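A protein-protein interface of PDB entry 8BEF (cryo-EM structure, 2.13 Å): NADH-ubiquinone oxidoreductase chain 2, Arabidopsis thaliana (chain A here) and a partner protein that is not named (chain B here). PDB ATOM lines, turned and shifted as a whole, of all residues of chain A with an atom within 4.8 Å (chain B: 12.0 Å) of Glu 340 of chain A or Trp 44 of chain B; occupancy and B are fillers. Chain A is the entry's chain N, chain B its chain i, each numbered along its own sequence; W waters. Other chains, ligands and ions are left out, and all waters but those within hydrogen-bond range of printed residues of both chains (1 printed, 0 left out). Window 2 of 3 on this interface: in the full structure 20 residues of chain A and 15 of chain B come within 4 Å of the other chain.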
ATOM      1  N   THR A 338       2.661 -26.660  -0.638  1.00  0.00           N
ATOM      2  CA  THR A 338       3.448 -25.895   0.319  1.00  0.00           C
ATOM      3  C   THR A 338       3.457 -24.431  -0.098  1.00  0.00           C
ATOM      4  O   THR A 338       3.135 -24.093  -1.238  1.00  0.00           O
ATOM      5  CB  THR A 338       4.893 -26.411   0.431  1.00  0.00           C
ATOM      6  OG1 THR A 338       5.593 -26.159  -0.794  1.00  0.00           O
ATOM      7  CG2 THR A 338       4.924 -27.897   0.738  1.00  0.00           C
ATOM      8  N   ILE A 339       3.719 -23.522   0.856  1.00  0.00           N
ATOM      9  CA  ILE A 339       3.922 -22.077   0.561  1.00  0.00           C
ATOM     10  C   ILE A 339       4.929 -21.902  -0.614  1.00  0.00           C
ATOM     11  O   ILE A 339       4.609 -21.181  -1.498  1.00  0.00           O
ATOM     12  CB  ILE A 339       4.325 -21.225   1.799  1.00  0.00           C
ATOM     13  CG1 ILE A 339       3.204 -21.127   2.825  1.00  0.00           C
ATOM     14  CG2 ILE A 339       4.767 -19.840   1.369  1.00  0.00           C
ATOM     15  CD1 ILE A 339       1.932 -20.562   2.277  1.00  0.00           C
ATOM     16  N   GLU A 340       6.048 -22.608  -0.637  1.00  0.00           N
ATOM     17  CA  GLU A 340       6.981 -22.500  -1.750  1.00  0.00           C
ATOM     18  C   GLU A 340       6.378 -23.049  -3.033  1.00  0.00           C
ATOM     19  O   GLU A 340       6.688 -22.550  -4.117  1.00  0.00           O
ATOM     20  CB  GLU A 340       8.310 -23.207  -1.443  1.00  0.00           C
ATOM     21  CG  GLU A 340       8.848 -23.105  -0.013  1.00  0.00           C
ATOM     22  CD  GLU A 340       7.967 -23.755   1.030  1.00  0.00           C
ATOM     23  OE1 GLU A 340       7.637 -24.945   0.863  1.00  0.00           O
ATOM     24  OE2 GLU A 340       7.593 -23.072   2.004  1.00  0.00           O
ATOM     25  N   GLY A 341       5.513 -24.060  -2.935  1.00  0.00           N
ATOM     26  CA  GLY A 341       4.835 -24.553  -4.125  1.00  0.00           C
ATOM     27  C   GLY A 341       3.971 -23.494  -4.784  1.00  0.00           C
ATOM     28  O   GLY A 341       4.026 -23.295  -6.000  1.00  0.00           O
ATOM     29  N   ILE A 342       3.174 -22.803  -3.980  1.00  0.00           N
ATOM     30  CA  ILE A 342       2.291 -21.710  -4.478  1.00  0.00           C
ATOM     31  C   ILE A 342       3.160 -20.586  -5.057  1.00  0.00           C
ATOM     32  O   ILE A 342       2.936 -20.239  -6.183  1.00  0.00           O
ATOM     33  CB  ILE A 342       1.265 -21.201  -3.435  1.00  0.00           C
ATOM     34  CG1 ILE A 342       0.107 -22.181  -3.260  1.00  0.00           C
ATOM     35  CG2 ILE A 342       0.734 -19.840  -3.824  1.00  0.00           C
ATOM     36  CD1 ILE A 342       0.496 -23.496  -2.696  1.00  0.00           C
ATOM     37  N   GLN A 343       4.214 -20.211  -4.333  1.00  0.00           N
ATOM     38  CA  GLN A 343       5.102 -19.155  -4.805  1.00  0.00           C
ATOM     39  C   GLN A 343       5.720 -19.516  -6.148  1.00  0.00           C
ATOM     40  O   GLN A 343       5.794 -18.680  -7.054  1.00  0.00           O
ATOM     41  CB  GLN A 343       6.195 -18.888  -3.775  1.00  0.00           C
ATOM     42  CG  GLN A 343       6.901 -17.569  -3.966  1.00  0.00           C
ATOM     43  CD  GLN A 343       8.238 -17.513  -3.256  1.00  0.00           C
ATOM     44  OE1 GLN A 343       8.672 -18.488  -2.646  1.00  0.00           O
ATOM     45  NE2 GLN A 343       8.904 -16.369  -3.341  1.00  0.00           N
ATOM     46  N   SER A 344       6.171 -20.761  -6.291  1.00  0.00           N
ATOM     47  CA  SER A 344       6.771 -21.199  -7.540  1.00  0.00           C
ATOM     48  C   SER A 344       5.749 -21.234  -8.665  1.00  0.00           C
ATOM     49  O   SER A 344       6.070 -20.894  -9.806  1.00  0.00           O
ATOM     50  CB  SER A 344       7.400 -22.570  -7.353  1.00  0.00           C
ATOM     51  OG  SER A 344       6.410 -23.517  -7.000  1.00  0.00           O
ATOM     52  N   TYR A 412      12.648 -25.013 -10.134  1.00  0.00           N
ATOM     53  CA  TYR A 412      11.634 -25.395  -9.157  1.00  0.00           C
ATOM     54  C   TYR A 412      11.084 -26.789  -9.420  1.00  0.00           C
ATOM     55  O   TYR A 412      10.746 -27.504  -8.474  1.00  0.00           O
ATOM     56  CB  TYR A 412      10.468 -24.416  -9.106  1.00  0.00           C
ATOM     57  CG  TYR A 412       9.433 -24.981  -8.162  1.00  0.00           C
ATOM     58  CD1 TYR A 412       9.642 -24.965  -6.788  1.00  0.00           C
ATOM     59  CD2 TYR A 412       8.297 -25.627  -8.645  1.00  0.00           C
ATOM     60  CE1 TYR A 412       8.721 -25.517  -5.920  1.00  0.00           C
ATOM     61  CE2 TYR A 412       7.378 -26.195  -7.783  1.00  0.00           C
ATOM     62  CZ  TYR A 412       7.594 -26.133  -6.421  1.00  0.00           C
ATOM     63  OH  TYR A 412       6.678 -26.684  -5.560  1.00  0.00           O
ATOM     64  N   PHE A 415      13.448 -28.889  -7.796  1.00  0.00           N
ATOM     65  CA  PHE A 415      13.424 -28.606  -6.360  1.00  0.00           C
ATOM     66  C   PHE A 415      12.254 -29.299  -5.675  1.00  0.00           C
ATOM     67  O   PHE A 415      12.409 -29.858  -4.586  1.00  0.00           O
ATOM     68  CB  PHE A 415      13.355 -27.096  -6.118  1.00  0.00           C
ATOM     69  CG  PHE A 415      13.804 -26.668  -4.741  1.00  0.00           C
ATOM     70  CD1 PHE A 415      12.887 -26.193  -3.819  1.00  0.00           C
ATOM     71  CD2 PHE A 415      15.135 -26.732  -4.372  1.00  0.00           C
ATOM     72  CE1 PHE A 415      13.288 -25.791  -2.556  1.00  0.00           C
ATOM     73  CE2 PHE A 415      15.541 -26.335  -3.109  1.00  0.00           C
ATOM     74  CZ  PHE A 415      14.615 -25.864  -2.201  1.00  0.00           C
ATOM     75  N   ARG B  36      25.038 -19.808  10.786  1.00  0.00           N
ATOM     76  CA  ARG B  36      23.982 -19.122  10.053  1.00  0.00           C
ATOM     77  C   ARG B  36      23.135 -20.062   9.202  1.00  0.00           C
ATOM     78  O   ARG B  36      22.094 -19.637   8.687  1.00  0.00           O
ATOM     79  CB  ARG B  36      24.574 -18.026   9.155  1.00  0.00           C
ATOM     80  CG  ARG B  36      23.619 -16.868   8.888  1.00  0.00           C
ATOM     81  CD  ARG B  36      24.178 -15.882   7.872  1.00  0.00           C
ATOM     82  NE  ARG B  36      24.190 -16.433   6.522  1.00  0.00           N
ATOM     83  CZ  ARG B  36      24.630 -15.787   5.451  1.00  0.00           C
ATOM     84  NH1 ARG B  36      25.110 -14.557   5.533  1.00  0.00           N
ATOM     85  NH2 ARG B  36      24.593 -16.393   4.267  1.00  0.00           N
ATOM     86  N   CYS B  37      23.547 -21.317   9.045  1.00  0.00           N
ATOM     87  CA  CYS B  37      22.797 -22.267   8.219  1.00  0.00           C
ATOM     88  C   CYS B  37      21.448 -22.709   8.832  1.00  0.00           C
ATOM     89  O   CYS B  37      20.846 -23.625   8.256  1.00  0.00           O
ATOM     90  CB  CYS B  37      23.661 -23.499   7.938  1.00  0.00           C
ATOM     91  SG  CYS B  37      23.706 -24.709   9.280  1.00  0.00           S
ATOM     92  N   LYS B  38      20.935 -22.146   9.927  1.00  0.00           N
ATOM     93  CA  LYS B  38      19.700 -22.635  10.532  1.00  0.00           C
ATOM     94  C   LYS B  38      18.474 -21.792  10.208  1.00  0.00           C
ATOM     95  O   LYS B  38      17.354 -22.311  10.254  1.00  0.00           O
ATOM     96  CB  LYS B  38      19.845 -22.708  12.057  1.00  0.00           C
ATOM     97  CG  LYS B  38      21.273 -22.632  12.566  1.00  0.00           C
ATOM     98  CD  LYS B  38      21.936 -23.998  12.560  1.00  0.00           C
ATOM     99  CE  LYS B  38      23.328 -23.933  13.163  1.00  0.00           C
ATOM    100  NZ  LYS B  38      23.831 -25.282  13.540  1.00  0.00           N
ATOM    101  N   LYS B  39      18.654 -20.510   9.885  1.00  0.00           N
ATOM    102  CA  LYS B  39      17.519 -19.592   9.814  1.00  0.00           C
ATOM    103  C   LYS B  39      16.592 -19.922   8.647  1.00  0.00           C
ATOM    104  O   LYS B  39      15.367 -19.966   8.809  1.00  0.00           O
ATOM    105  CB  LYS B  39      18.025 -18.153   9.705  1.00  0.00           C
ATOM    106  CG  LYS B  39      18.709 -17.637  10.964  1.00  0.00           C
ATOM    107  CD  LYS B  39      18.864 -16.121  10.951  1.00  0.00           C
ATOM    108  CE  LYS B  39      17.744 -15.437  10.178  1.00  0.00           C
ATOM    109  NZ  LYS B  39      16.436 -15.522  10.888  1.00  0.00           N
ATOM    110  N   ILE B  40      17.159 -20.151   7.463  1.00  0.00           N
ATOM    111  CA  ILE B  40      16.343 -20.289   6.259  1.00  0.00           C
ATOM    112  C   ILE B  40      15.535 -21.580   6.288  1.00  0.00           C
ATOM    113  O   ILE B  40      14.383 -21.615   5.839  1.00  0.00           O
ATOM    114  CB  ILE B  40      17.233 -20.197   5.009  1.00  0.00           C
ATOM    115  CG1 ILE B  40      18.008 -18.883   5.031  1.00  0.00           C
ATOM    116  CG2 ILE B  40      16.398 -20.306   3.743  1.00  0.00           C
ATOM    117  CD1 ILE B  40      17.125 -17.657   5.119  1.00  0.00           C
ATOM    118  N   LYS B  41      16.119 -22.660   6.812  1.00  0.00           N
ATOM    119  CA  LYS B  41      15.421 -23.942   6.840  1.00  0.00           C
ATOM    120  C   LYS B  41      14.168 -23.903   7.707  1.00  0.00           C
ATOM    121  O   LYS B  41      13.311 -24.783   7.576  1.00  0.00           O
ATOM    122  CB  LYS B  41      16.367 -25.040   7.329  1.00  0.00           C
ATOM    123  CG  LYS B  41      16.848 -25.971   6.227  1.00  0.00           C
ATOM    124  CD  LYS B  41      17.615 -27.152   6.795  1.00  0.00           C
ATOM    125  CE  LYS B  41      19.037 -26.760   7.161  1.00  0.00           C
ATOM    126  NZ  LYS B  41      19.862 -26.472   5.954  1.00  0.00           N
ATOM    127  N   GLU B  42      14.040 -22.904   8.584  1.00  0.00           N
ATOM    128  CA  GLU B  42      12.830 -22.779   9.391  1.00  0.00           C
ATOM    129  C   GLU B  42      11.651 -22.280   8.565  1.00  0.00           C
ATOM    130  O   GLU B  42      10.504 -22.654   8.837  1.00  0.00           O
ATOM    131  CB  GLU B  42      13.084 -21.846  10.575  1.00  0.00           C
ATOM    132  CG  GLU B  42      14.097 -22.377  11.577  1.00  0.00           C
ATOM    133  CD  GLU B  42      13.443 -23.038  12.774  1.00  0.00           C
ATOM    134  OE1 GLU B  42      12.199 -23.151  12.787  1.00  0.00           O
ATOM    135  OE2 GLU B  42      14.174 -23.442  13.703  1.00  0.00           O
ATOM    136  N   MET B  43      11.907 -21.431   7.567  1.00  0.00           N
ATOM    137  CA  MET B  43      10.829 -20.956   6.702  1.00  0.00           C
ATOM    138  C   MET B  43      10.280 -22.080   5.835  1.00  0.00           C
ATOM    139  O   MET B  43       9.072 -22.146   5.585  1.00  0.00           O
ATOM    140  CB  MET B  43      11.326 -19.799   5.836  1.00  0.00           C
ATOM    141  CG  MET B  43      10.313 -18.684   5.632  1.00  0.00           C
ATOM    142  SD  MET B  43      10.779 -17.584   4.283  1.00  0.00           S
ATOM    143  CE  MET B  43      11.893 -16.463   5.124  1.00  0.00           C
ATOM    144  N   TRP B  44      11.153 -22.978   5.367  1.00  0.00           N
ATOM    145  CA  TRP B  44      10.712 -24.093   4.538  1.00  0.00           C
ATOM    146  C   TRP B  44       9.836 -25.076   5.305  1.00  0.00           C
ATOM    147  O   TRP B  44       9.108 -25.855   4.682  1.00  0.00           O
ATOM    148  CB  TRP B  44      11.924 -24.817   3.945  1.00  0.00           C
ATOM    149  CG  TRP B  44      12.503 -24.127   2.743  1.00  0.00           C
ATOM    150  CD1 TRP B  44      11.888 -23.192   1.964  1.00  0.00           C
ATOM    151  CD2 TRP B  44      13.814 -24.309   2.191  1.00  0.00           C
ATOM    152  NE1 TRP B  44      12.730 -22.784   0.959  1.00  0.00           N
ATOM    153  CE2 TRP B  44      13.918 -23.456   1.074  1.00  0.00           C
ATOM    154  CE3 TRP B  44      14.906 -25.116   2.527  1.00  0.00           C
ATOM    155  CZ2 TRP B  44      15.070 -23.381   0.298  1.00  0.00           C
ATOM    156  CZ3 TRP B  44      16.048 -25.042   1.754  1.00  0.00           C
ATOM    157  CH2 TRP B  44      16.122 -24.179   0.652  1.00  0.00           C
ATOM    158  N   ALA B  45       9.888 -25.057   6.635  1.00  0.00           N
ATOM    159  CA  ALA B  45       9.046 -25.908   7.463  1.00  0.00           C
ATOM    160  C   ALA B  45       7.756 -25.225   7.901  1.00  0.00           C
ATOM    161  O   ALA B  45       6.962 -25.841   8.620  1.00  0.00           O
ATOM    162  CB  ALA B  45       9.822 -26.377   8.699  1.00  0.00           C
ATOM    163  N   LEU B  46       7.530 -23.981   7.491  1.00  0.00           N
ATOM    164  CA  LEU B  46       6.313 -23.276   7.877  1.00  0.00           C
ATOM    165  C   LEU B  46       5.103 -23.951   7.243  1.00  0.00           C
ATOM    166  O   LEU B  46       5.113 -24.225   6.036  1.00  0.00           O
ATOM    167  CB  LEU B  46       6.381 -21.810   7.449  1.00  0.00           C
ATOM    168  CG  LEU B  46       6.570 -20.765   8.552  1.00  0.00           C
ATOM    169  CD1 LEU B  46       6.899 -19.409   7.951  1.00  0.00           C
ATOM    170  CD2 LEU B  46       5.337 -20.671   9.432  1.00  0.00           C
ATOM    171  N   PRO B  47       4.055 -24.243   8.010  1.00  0.00           N
ATOM    172  CA  PRO B  47       2.887 -24.920   7.432  1.00  0.00           C
ATOM    173  C   PRO B  47       2.194 -24.049   6.396  1.00  0.00           C
ATOM    174  O   PRO B  47       2.003 -22.847   6.593  1.00  0.00           O
ATOM    175  CB  PRO B  47       1.991 -25.173   8.650  1.00  0.00           C
ATOM    176  CG  PRO B  47       2.388 -24.116   9.622  1.00  0.00           C
ATOM    177  CD  PRO B  47       3.871 -23.968   9.444  1.00  0.00           C
ATOM    178  N   ILE B  48       1.740 -24.612   5.292  1.00  0.00           N
ATOM    179  CA  ILE B  48       1.004 -23.792   4.311  1.00  0.00           C
ATOM    180  C   ILE B  48      -0.411 -23.572   4.865  1.00  0.00           C
ATOM    181  O   ILE B  48      -1.014 -22.517   4.563  1.00  0.00           O
ATOM    182  CB  ILE B  48       1.037 -24.534   2.955  1.00  0.00           C
ATOM    183  CG1 ILE B  48       0.342 -23.793   1.816  1.00  0.00           C
ATOM    184  CG2 ILE B  48       0.472 -25.939   3.111  1.00  0.00           C
ATOM    185  CD1 ILE B  48       0.148 -24.661   0.603  1.00  0.00           C
ATOM    186  N   ARG B  49      -0.910 -24.558   5.622  1.00  0.00           N
ATOM    187  CA  ARG B  49      -2.204 -24.380   6.267  1.00  0.00           C
ATOM    188  C   ARG B  49      -1.959 -24.057   7.732  1.00  0.00           C
ATOM    189  O   ARG B  49      -1.650 -24.962   8.524  1.00  0.00           O
ATOM    190  CB  ARG B  49      -3.047 -25.651   6.117  1.00  0.00           C
ATOM    191  CG  ARG B  49      -4.512 -25.524   6.490  1.00  0.00           C
ATOM    192  CD  ARG B  49      -4.733 -25.854   7.959  1.00  0.00           C
ATOM    193  NE  ARG B  49      -4.355 -27.227   8.273  1.00  0.00           N
ATOM    194  CZ  ARG B  49      -4.381 -27.749   9.492  1.00  0.00           C
ATOM    195  NH1 ARG B  49      -4.770 -27.041  10.539  1.00  0.00           N
ATOM    196  NH2 ARG B  49      -4.009 -29.015   9.663  1.00  0.00           N
ATOM    197  N   PRO B  50      -2.058 -22.756   8.118  1.00  0.00           N
ATOM    198  CA  PRO B  50      -1.757 -22.403   9.494  1.00  0.00           C
ATOM    199  C   PRO B  50      -2.707 -23.075  10.498  1.00  0.00           C
ATOM    200  O   PRO B  50      -3.719 -23.585  10.089  1.00  0.00           O
ATOM    201  CB  PRO B  50      -1.838 -20.861   9.426  1.00  0.00           C
ATOM    202  CG  PRO B  50      -2.810 -20.552   8.355  1.00  0.00           C
ATOM    203  CD  PRO B  50      -2.446 -21.574   7.320  1.00  0.00           C
HETATM  204  O   HOH W   1       5.156 -24.384   2.848  1.00  0.00           O
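Among the printed residues, merely in contact across the chains: Thr 338 of chain A with Ile 48 of chain B, Ile 342 of chain A with Ile 48 of chain B, Ile 339 of chain A with Ile 48 of chain B, Phe 415 of chain A with Trp 44 of chain B, Glu 340 of chain A with Trp 44 of chain B and Glu 340 of chain A with Met 43 of chain B.
Thr 338 of chain A touches just one residue of chain B: Ile 48 (3.4 Å). Ile 339 of chain A touches just one residue of chain B: Ile 48 (3.5 Å). Printed residues of chain B within 4 Å of Glu 340 of chain A: Met 43 (3.98 Å) and Trp 44 (3.6 Å). No residue of chain B comes within 4 Å of Gln 343 of chain A. Of the printed residues of chain B, Phe 415 of chain A touches Trp 44 (3.6 Å). Of the printed residues of chain A, Met 43 of chain B touches Glu 340. Of chain A, only Glu 340 (3.6 Å) and Phe 415 (3.6 Å) come within 4 Å of Trp 44 of chain B. Printed residues of chain A within 4 Å of Ile 48 of chain B: Thr 338 (3.4 Å), Ile 339 (3.5 Å) and Ile 342 (3.5 Å). The nearest printed residue of chain B that does not touch Glu 340 of chain A is Leu 46 of chain B (4.9 Å). The nearest printed residue of chain B that does not touch Phe 415 of chain A is Ile 40 of chain B (8.3 Å).
Water W1 lies within hydrogen-bond range of the backbone NH (N) of Ile 339 of chain A (2.6 Å), the side-chain carboxylate (OE2) of Glu 340 of chain A (2.9 Å) and the backbone carbonyl oxygen (O) of Leu 46 of chain B (3.2 Å).
Of the 15 printed residues of chain B, 3 touch a printed residue of chain A. Of the 9 printed residues of chain A, 5 touch a printed residue of chain B. Printed residues of chain A that touch a printed residue of chain B: Thr 338, Ile 339, Glu 340, Ile 342 and Phe 415.
The side-chain hydroxyl (OG1) of Thr 338 of chain A is in hydrogen-bond range of the side-chain carboxylate (OE1) of Glu 340 of chain A (2.9 Å). The side-chain hydroxyl (OG1) of Thr 338 of chain A lies within hydrogen-bond range of the backbone NH (N) of Gly 341 of chain A (3.0 Å). O of Glu 340 of chain A lies within hydrogen-bond range of OG of Ser 344 of chain A (3.1 Å).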
